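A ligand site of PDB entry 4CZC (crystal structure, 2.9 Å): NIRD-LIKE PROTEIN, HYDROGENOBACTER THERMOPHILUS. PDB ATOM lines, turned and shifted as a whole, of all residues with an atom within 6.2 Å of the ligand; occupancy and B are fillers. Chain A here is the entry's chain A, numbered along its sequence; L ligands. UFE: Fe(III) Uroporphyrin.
The guanidinium group (NH1) of Arg 218 lies within salt-bridge range of an oxygen (O4A) of the ligand (3.5 Å).
An iron atom (FE) of the ligand is bound by a ring nitrogen (NE2) of His 261.
The side-chain hydroxyl (OH) of Tyr 263 sits at hydrogen-bond distance from an oxygen (O1D) of the ligand (3.2 Å).
OD1 of Asn 234 lies close to O1C of the ligand (3.5 Å).
NE2 of His 93 sits at hydrogen-bond distance from O4D of the ligand (3.0 Å).
Residues that only touch the ligand: Arg 139 (3.6 Å), Ser 260 (3.7 Å) and Met 278 (3.2 Å).
Hydrophobic or aromatic side chains that line the ligand: His 93, His 261 and Met 278.
Within 4 Å of the ligand: His 93, Arg 139, Arg 218, Asn 234, Ser 260, His 261, Tyr 263 and Met 278.
Along chain A the residues within 4 Å of the ligand span positions 93 to 278.
The nearest printed residue that does not touch the ligand is Ile 56 (4.2 Å).
O of His 261 lies within hydrogen-bond range of N of Met 278 (3.1 Å).
The backbone carbonyl oxygen (O) of Met 278 sits at hydrogen-bond distance from the backbone NH (N) of Ser 260, at 2.9 Å.
The backbone NH (N) of Arg 218 sits at hydrogen-bond distance from the backbone carbonyl oxygen (O) of Ile 56, 2.8 Å away.
The side-chain amide nitrogen of Asn 234 lies close to the backbone NH of Val 232 (3.0 Å).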
ATOM      1  N   ILE A  56     -31.253 -10.759  -3.836  1.00  0.00           N
ATOM      2  CA  ILE A  56     -30.003 -11.172  -3.289  1.00  0.00           C
ATOM      3  C   ILE A  56     -29.994 -10.546  -1.926  1.00  0.00           C
ATOM      4  O   ILE A  56     -30.060  -9.304  -1.846  1.00  0.00           O
ATOM      5  CB  ILE A  56     -28.836 -10.669  -4.125  1.00  0.00           C
ATOM      6  CG1 ILE A  56     -28.482 -11.688  -5.222  1.00  0.00           C
ATOM      7  CG2 ILE A  56     -27.598 -10.529  -3.261  1.00  0.00           C
ATOM      8  CD1 ILE A  56     -29.530 -11.991  -6.289  1.00  0.00           C
ATOM      9  N   SER A  92     -23.484 -25.261   1.237  1.00  0.00           N
ATOM     10  CA  SER A  92     -23.802 -24.787  -0.124  1.00  0.00           C
ATOM     11  C   SER A  92     -22.903 -25.466  -1.123  1.00  0.00           C
ATOM     12  O   SER A  92     -23.369 -25.962  -2.124  1.00  0.00           O
ATOM     13  CB  SER A  92     -23.654 -23.252  -0.237  1.00  0.00           C
ATOM     14  OG  SER A  92     -22.426 -22.791   0.308  1.00  0.00           O
ATOM     15  N   HIS A  93     -21.606 -25.441  -0.861  1.00  0.00           N
ATOM     16  CA  HIS A  93     -20.616 -26.089  -1.707  1.00  0.00           C
ATOM     17  C   HIS A  93     -19.930 -27.213  -0.949  1.00  0.00           C
ATOM     18  O   HIS A  93     -19.809 -27.183   0.274  1.00  0.00           O
ATOM     19  CB  HIS A  93     -19.594 -25.087  -2.182  1.00  0.00           C
ATOM     20  CG  HIS A  93     -20.198 -23.885  -2.828  1.00  0.00           C
ATOM     21  ND1 HIS A  93     -20.447 -23.831  -4.179  1.00  0.00           N
ATOM     22  CD2 HIS A  93     -20.623 -22.710  -2.312  1.00  0.00           C
ATOM     23  CE1 HIS A  93     -21.004 -22.663  -4.478  1.00  0.00           C
ATOM     24  NE2 HIS A  93     -21.118 -21.974  -3.362  1.00  0.00           N
ATOM     25  N   ARG A 139     -14.651 -11.712   0.936  1.00  0.00           N
ATOM     26  CA  ARG A 139     -14.390 -11.337  -0.451  1.00  0.00           C
ATOM     27  C   ARG A 139     -13.948  -9.878  -0.601  1.00  0.00           C
ATOM     28  O   ARG A 139     -13.709  -9.194   0.386  1.00  0.00           O
ATOM     29  CB  ARG A 139     -15.619 -11.621  -1.327  1.00  0.00           C
ATOM     30  CG  ARG A 139     -16.912 -11.059  -0.793  1.00  0.00           C
ATOM     31  CD  ARG A 139     -16.977  -9.535  -0.915  1.00  0.00           C
ATOM     32  NE  ARG A 139     -18.352  -9.037  -0.867  1.00  0.00           N
ATOM     33  CZ  ARG A 139     -19.101  -8.757  -1.925  1.00  0.00           C
ATOM     34  NH1 ARG A 139     -18.619  -8.917  -3.157  1.00  0.00           N
ATOM     35  NH2 ARG A 139     -20.340  -8.314  -1.762  1.00  0.00           N
ATOM     36  N   ARG A 218     -29.727  -6.689  -0.766  1.00  0.00           N
ATOM     37  CA  ARG A 218     -28.764  -5.983  -1.601  1.00  0.00           C
ATOM     38  C   ARG A 218     -29.478  -5.439  -2.819  1.00  0.00           C
ATOM     39  O   ARG A 218     -29.451  -4.235  -3.095  1.00  0.00           O
ATOM     40  CB  ARG A 218     -27.640  -6.903  -2.053  1.00  0.00           C
ATOM     41  CG  ARG A 218     -26.518  -7.155  -1.049  1.00  0.00           C
ATOM     42  CD  ARG A 218     -25.263  -7.537  -1.846  1.00  0.00           C
ATOM     43  NE  ARG A 218     -24.143  -7.918  -0.993  1.00  0.00           N
ATOM     44  CZ  ARG A 218     -23.705  -9.171  -0.790  1.00  0.00           C
ATOM     45  NH1 ARG A 218     -24.268 -10.217  -1.412  1.00  0.00           N
ATOM     46  NH2 ARG A 218     -22.673  -9.370   0.031  1.00  0.00           N
ATOM     47  N   ARG A 219     -30.141  -6.341  -3.537  1.00  0.00           N
ATOM     48  CA  ARG A 219     -30.775  -5.993  -4.779  1.00  0.00           C
ATOM     49  C   ARG A 219     -31.702  -7.126  -5.209  1.00  0.00           C
ATOM     50  O   ARG A 219     -31.665  -8.213  -4.646  1.00  0.00           O
ATOM     51  CB  ARG A 219     -29.682  -5.812  -5.822  1.00  0.00           C
ATOM     52  CG  ARG A 219     -28.881  -7.102  -5.999  1.00  0.00           C
ATOM     53  CD  ARG A 219     -27.446  -6.876  -6.416  1.00  0.00           C
ATOM     54  NE  ARG A 219     -27.473  -6.229  -7.703  1.00  0.00           N
ATOM     55  CZ  ARG A 219     -27.522  -6.849  -8.870  1.00  0.00           C
ATOM     56  NH1 ARG A 219     -27.519  -8.185  -8.951  1.00  0.00           N
ATOM     57  NH2 ARG A 219     -27.567  -6.120  -9.983  1.00  0.00           N
ATOM     58  N   VAL A 232     -14.523 -26.832 -14.951  1.00  0.00           N
ATOM     59  CA  VAL A 232     -13.513 -26.975 -15.993  1.00  0.00           C
ATOM     60  C   VAL A 232     -12.262 -27.631 -15.401  1.00  0.00           C
ATOM     61  O   VAL A 232     -12.155 -28.845 -15.339  1.00  0.00           O
ATOM     62  CB  VAL A 232     -13.151 -25.608 -16.615  1.00  0.00           C
ATOM     63  CG1 VAL A 232     -12.683 -25.809 -18.055  1.00  0.00           C
ATOM     64  CG2 VAL A 232     -14.331 -24.651 -16.551  1.00  0.00           C
ATOM     65  N   ASN A 234     -10.077 -26.531 -11.883  1.00  0.00           N
ATOM     66  CA  ASN A 234     -10.305 -25.494 -10.906  1.00  0.00           C
ATOM     67  C   ASN A 234      -9.456 -25.723  -9.677  1.00  0.00           C
ATOM     68  O   ASN A 234      -9.231 -26.861  -9.265  1.00  0.00           O
ATOM     69  CB  ASN A 234     -11.778 -25.434 -10.526  1.00  0.00           C
ATOM     70  CG  ASN A 234     -12.676 -25.014 -11.690  1.00  0.00           C
ATOM     71  OD1 ASN A 234     -13.002 -23.842 -11.845  1.00  0.00           O
ATOM     72  ND2 ASN A 234     -13.055 -25.971 -12.524  1.00  0.00           N
ATOM     73  N   ALA A 254      -6.514 -10.107  -8.962  1.00  0.00           N
ATOM     74  CA  ALA A 254      -7.882  -9.871  -9.483  1.00  0.00           C
ATOM     75  C   ALA A 254      -7.892  -9.394 -10.944  1.00  0.00           C
ATOM     76  O   ALA A 254      -8.929  -9.465 -11.594  1.00  0.00           O
ATOM     77  CB  ALA A 254      -8.610  -8.865  -8.610  1.00  0.00           C
ATOM     78  N   VAL A 259      -8.323 -16.110 -12.785  1.00  0.00           N
ATOM     79  CA  VAL A 259      -8.600 -15.763 -11.404  1.00  0.00           C
ATOM     80  C   VAL A 259      -9.963 -15.109 -11.346  1.00  0.00           C
ATOM     81  O   VAL A 259     -10.194 -14.079 -12.000  1.00  0.00           O
ATOM     82  CB  VAL A 259      -7.579 -14.747 -10.881  1.00  0.00           C
ATOM     83  CG1 VAL A 259      -7.958 -14.262  -9.492  1.00  0.00           C
ATOM     84  CG2 VAL A 259      -6.194 -15.355 -10.880  1.00  0.00           C
ATOM     85  N   SER A 260     -10.843 -15.665 -10.512  1.00  0.00           N
ATOM     86  CA  SER A 260     -12.187 -15.089 -10.303  1.00  0.00           C
ATOM     87  C   SER A 260     -12.448 -14.150  -9.105  1.00  0.00           C
ATOM     88  O   SER A 260     -12.498 -12.932  -9.267  1.00  0.00           O
ATOM     89  CB  SER A 260     -13.204 -16.206 -10.187  1.00  0.00           C
ATOM     90  OG  SER A 260     -12.779 -17.162  -9.245  1.00  0.00           O
ATOM     91  N   HIS A 261     -12.662 -14.721  -7.927  1.00  0.00           N
ATOM     92  CA  HIS A 261     -12.833 -13.880  -6.757  1.00  0.00           C
ATOM     93  C   HIS A 261     -11.596 -14.036  -5.870  1.00  0.00           C
ATOM     94  O   HIS A 261     -10.944 -15.085  -5.890  1.00  0.00           O
ATOM     95  CB  HIS A 261     -14.128 -14.201  -5.997  1.00  0.00           C
ATOM     96  CG  HIS A 261     -15.349 -13.946  -6.788  1.00  0.00           C
ATOM     97  ND1 HIS A 261     -15.768 -12.677  -7.112  1.00  0.00           N
ATOM     98  CD2 HIS A 261     -16.249 -14.797  -7.306  1.00  0.00           C
ATOM     99  CE1 HIS A 261     -16.877 -12.762  -7.826  1.00  0.00           C
ATOM    100  NE2 HIS A 261     -17.188 -14.047  -7.952  1.00  0.00           N
ATOM    101  N   TYR A 263     -10.280 -13.601  -1.717  1.00  0.00           N
ATOM    102  CA  TYR A 263     -10.748 -13.577  -0.307  1.00  0.00           C
ATOM    103  C   TYR A 263      -9.611 -13.462   0.702  1.00  0.00           C
ATOM    104  O   TYR A 263      -8.509 -13.908   0.437  1.00  0.00           O
ATOM    105  CB  TYR A 263     -11.520 -14.841   0.018  1.00  0.00           C
ATOM    106  CG  TYR A 263     -12.556 -15.238  -0.985  1.00  0.00           C
ATOM    107  CD1 TYR A 263     -12.192 -15.911  -2.138  1.00  0.00           C
ATOM    108  CD2 TYR A 263     -13.892 -14.978  -0.758  1.00  0.00           C
ATOM    109  CE1 TYR A 263     -13.141 -16.310  -3.049  1.00  0.00           C
ATOM    110  CE2 TYR A 263     -14.854 -15.373  -1.666  1.00  0.00           C
ATOM    111  CZ  TYR A 263     -14.479 -16.027  -2.801  1.00  0.00           C
ATOM    112  OH  TYR A 263     -15.426 -16.413  -3.727  1.00  0.00           O
ATOM    113  N   MET A 278      -9.500 -17.786  -6.144  1.00  0.00           N
ATOM    114  CA  MET A 278     -10.163 -18.862  -6.863  1.00  0.00           C
ATOM    115  C   MET A 278      -9.677 -18.888  -8.258  1.00  0.00           C
ATOM    116  O   MET A 278      -9.748 -17.883  -8.945  1.00  0.00           O
ATOM    117  CB  MET A 278     -11.668 -18.630  -6.877  1.00  0.00           C
ATOM    118  CG  MET A 278     -12.235 -18.833  -5.488  1.00  0.00           C
ATOM    119  SD  MET A 278     -11.649 -20.517  -4.638  1.00  0.00           S
ATOM    120  CE  MET A 278     -10.542 -19.583  -3.294  1.00  0.00           C
ATOM    121  N   HIS A 280      -9.061 -21.024 -12.138  1.00  0.00           N
ATOM    122  CA  HIS A 280      -9.554 -21.987 -13.103  1.00  0.00           C
ATOM    123  C   HIS A 280      -8.779 -21.936 -14.418  1.00  0.00           C
ATOM    124  O   HIS A 280      -8.142 -20.927 -14.738  1.00  0.00           O
ATOM    125  CB  HIS A 280     -11.024 -21.732 -13.383  1.00  0.00           C
ATOM    126  CG  HIS A 280     -11.302 -20.345 -13.881  1.00  0.00           C
ATOM    127  ND1 HIS A 280     -10.838 -19.889 -15.097  1.00  0.00           N
ATOM    128  CD2 HIS A 280     -12.003 -19.323 -13.337  1.00  0.00           C
ATOM    129  CE1 HIS A 280     -11.230 -18.632 -15.277  1.00  0.00           C
ATOM    130  NE2 HIS A 280     -11.938 -18.268 -14.224  1.00  0.00           N
ATOM    131  N   LYS A 314     -23.250 -28.219  -5.415  1.00  0.00           N
ATOM    132  CA  LYS A 314     -23.186 -26.790  -5.709  1.00  0.00           C
ATOM    133  C   LYS A 314     -24.594 -26.218  -5.832  1.00  0.00           C
ATOM    134  O   LYS A 314     -25.052 -25.914  -6.928  1.00  0.00           O
ATOM    135  CB  LYS A 314     -22.407 -26.578  -7.022  1.00  0.00           C
ATOM    136  CG  LYS A 314     -22.102 -25.126  -7.334  1.00  0.00           C
ATOM    137  CD  LYS A 314     -21.675 -24.945  -8.804  1.00  0.00           C
ATOM    138  CE  LYS A 314     -20.801 -23.716  -9.024  1.00  0.00           C
ATOM    139  NZ  LYS A 314     -21.210 -22.509  -8.240  1.00  0.00           N
HETATM  140  O4D UFE L   1     -21.747 -19.095  -3.131  1.00  0.00           O
HETATM  141  CED UFE L   1     -21.211 -18.698  -4.201  1.00  0.00           C
HETATM  142  O3D UFE L   1     -21.324 -19.277  -5.308  1.00  0.00           O
HETATM  143  CDD UFE L   1     -20.407 -17.430  -4.101  1.00  0.00           C
HETATM  144  C3D UFE L   1     -19.748 -17.062  -5.405  1.00  0.00           C
HETATM  145  C2D UFE L   1     -18.827 -17.888  -6.209  1.00  0.00           C
HETATM  146  CAD UFE L   1     -18.358 -19.292  -5.897  1.00  0.00           C
HETATM  147  CBD UFE L   1     -16.893 -19.286  -5.423  1.00  0.00           C
HETATM  148  CCD UFE L   1     -16.001 -18.949  -6.591  1.00  0.00           C
HETATM  149  O2D UFE L   1     -16.217 -19.597  -7.637  1.00  0.00           O
HETATM  150  O1D UFE L   1     -15.135 -18.039  -6.506  1.00  0.00           O
HETATM  151  C1D UFE L   1     -18.503 -16.985  -7.347  1.00  0.00           C
HETATM  152  CHD UFE L   1     -17.624 -17.410  -8.467  1.00  0.00           C
HETATM  153  C4D UFE L   1     -19.851 -15.789  -6.187  1.00  0.00           C
HETATM  154  CHA UFE L   1     -20.659 -14.630  -5.718  1.00  0.00           C
HETATM  155  ND  UFE L   1     -19.136 -15.801  -7.320  1.00  0.00           N
HETATM  156 FE   UFE L   1     -18.913 -14.226  -8.676  1.00  0.00          FE
HETATM  157  NA  UFE L   1     -19.843 -12.942  -7.313  1.00  0.00           N
HETATM  158  C4A UFE L   1     -19.844 -11.609  -7.359  1.00  0.00           C
HETATM  159  C3A UFE L   1     -20.545 -10.950  -6.259  1.00  0.00           C
HETATM  160  CAA UFE L   1     -20.731  -9.486  -6.063  1.00  0.00           C
HETATM  161  CBA UFE L   1     -21.796  -9.076  -7.062  1.00  0.00           C
HETATM  162  CCA UFE L   1     -21.858  -7.573  -6.995  1.00  0.00           C
HETATM  163  O2A UFE L   1     -21.959  -6.904  -8.061  1.00  0.00           O
HETATM  164  O1A UFE L   1     -21.802  -7.020  -5.863  1.00  0.00           O
HETATM  165  C2A UFE L   1     -21.002 -12.067  -5.423  1.00  0.00           C
HETATM  166  CDA UFE L   1     -21.813 -11.992  -4.158  1.00  0.00           C
HETATM  167  CEA UFE L   1     -23.245 -11.802  -4.620  1.00  0.00           C
HETATM  168  O4A UFE L   1     -23.655 -10.629  -4.813  1.00  0.00           O
HETATM  169  O3A UFE L   1     -23.946 -12.836  -4.803  1.00  0.00           O
HETATM  170  C1A UFE L   1     -20.510 -13.246  -6.184  1.00  0.00           C
HETATM  171  NB  UFE L   1     -18.629 -12.618  -9.980  1.00  0.00           N
HETATM  172  C4B UFE L   1     -18.165 -12.644 -11.226  1.00  0.00           C
HETATM  173  C3B UFE L   1     -18.012 -11.295 -11.863  1.00  0.00           C
HETATM  174  CAB UFE L   1     -17.536 -10.975 -13.262  1.00  0.00           C
HETATM  175  CBB UFE L   1     -16.113 -11.517 -13.442  1.00  0.00           C
HETATM  176  CCB UFE L   1     -15.034 -10.655 -12.823  1.00  0.00           C
HETATM  177  O2B UFE L   1     -15.132  -9.404 -12.904  1.00  0.00           O
HETATM  178  O1B UFE L   1     -14.057 -11.221 -12.261  1.00  0.00           O
HETATM  179  C2B UFE L   1     -18.440 -10.347 -10.815  1.00  0.00           C
HETATM  180  CDB UFE L   1     -18.499  -8.813 -10.897  1.00  0.00           C
HETATM  181  CEB UFE L   1     -18.887  -8.075  -9.602  1.00  0.00           C
HETATM  182  O4B UFE L   1     -18.113  -7.199  -9.144  1.00  0.00           O
HETATM  183  O3B UFE L   1     -19.978  -8.336  -9.024  1.00  0.00           O
HETATM  184  C1B UFE L   1     -18.764 -11.296  -9.706  1.00  0.00           C
HETATM  185  CHB UFE L   1     -19.267 -10.818  -8.422  1.00  0.00           C
HETATM  186  NC  UFE L   1     -17.924 -15.493 -10.003  1.00  0.00           N
HETATM  187  C4C UFE L   1     -17.425 -16.707  -9.755  1.00  0.00           C
HETATM  188  C3C UFE L   1     -16.735 -17.315 -10.920  1.00  0.00           C
HETATM  189  C2C UFE L   1     -16.802 -16.256 -11.929  1.00  0.00           C
HETATM  190  CDC UFE L   1     -16.360 -16.149 -13.355  1.00  0.00           C
HETATM  191  CEC UFE L   1     -17.679 -15.922 -14.129  1.00  0.00           C
HETATM  192  O4C UFE L   1     -18.009 -14.761 -14.504  1.00  0.00           O
HETATM  193  O3C UFE L   1     -18.435 -16.892 -14.355  1.00  0.00           O
HETATM  194  C1C UFE L   1     -17.557 -15.198 -11.231  1.00  0.00           C
HETATM  195  CHC UFE L   1     -17.818 -13.906 -11.889  1.00  0.00           C
HETATM  196  CAC UFE L   1     -16.070 -18.653 -11.048  1.00  0.00           C
HETATM  197  CBC UFE L   1     -17.017 -19.759 -11.440  1.00  0.00           C
HETATM  198  CCC UFE L   1     -16.162 -20.904 -11.959  1.00  0.00           C
HETATM  199  O1C UFE L   1     -15.643 -21.711 -11.141  1.00  0.00           O
HETATM  200  O2C UFE L   1     -15.967 -21.003 -13.196  1.00  0.00           O
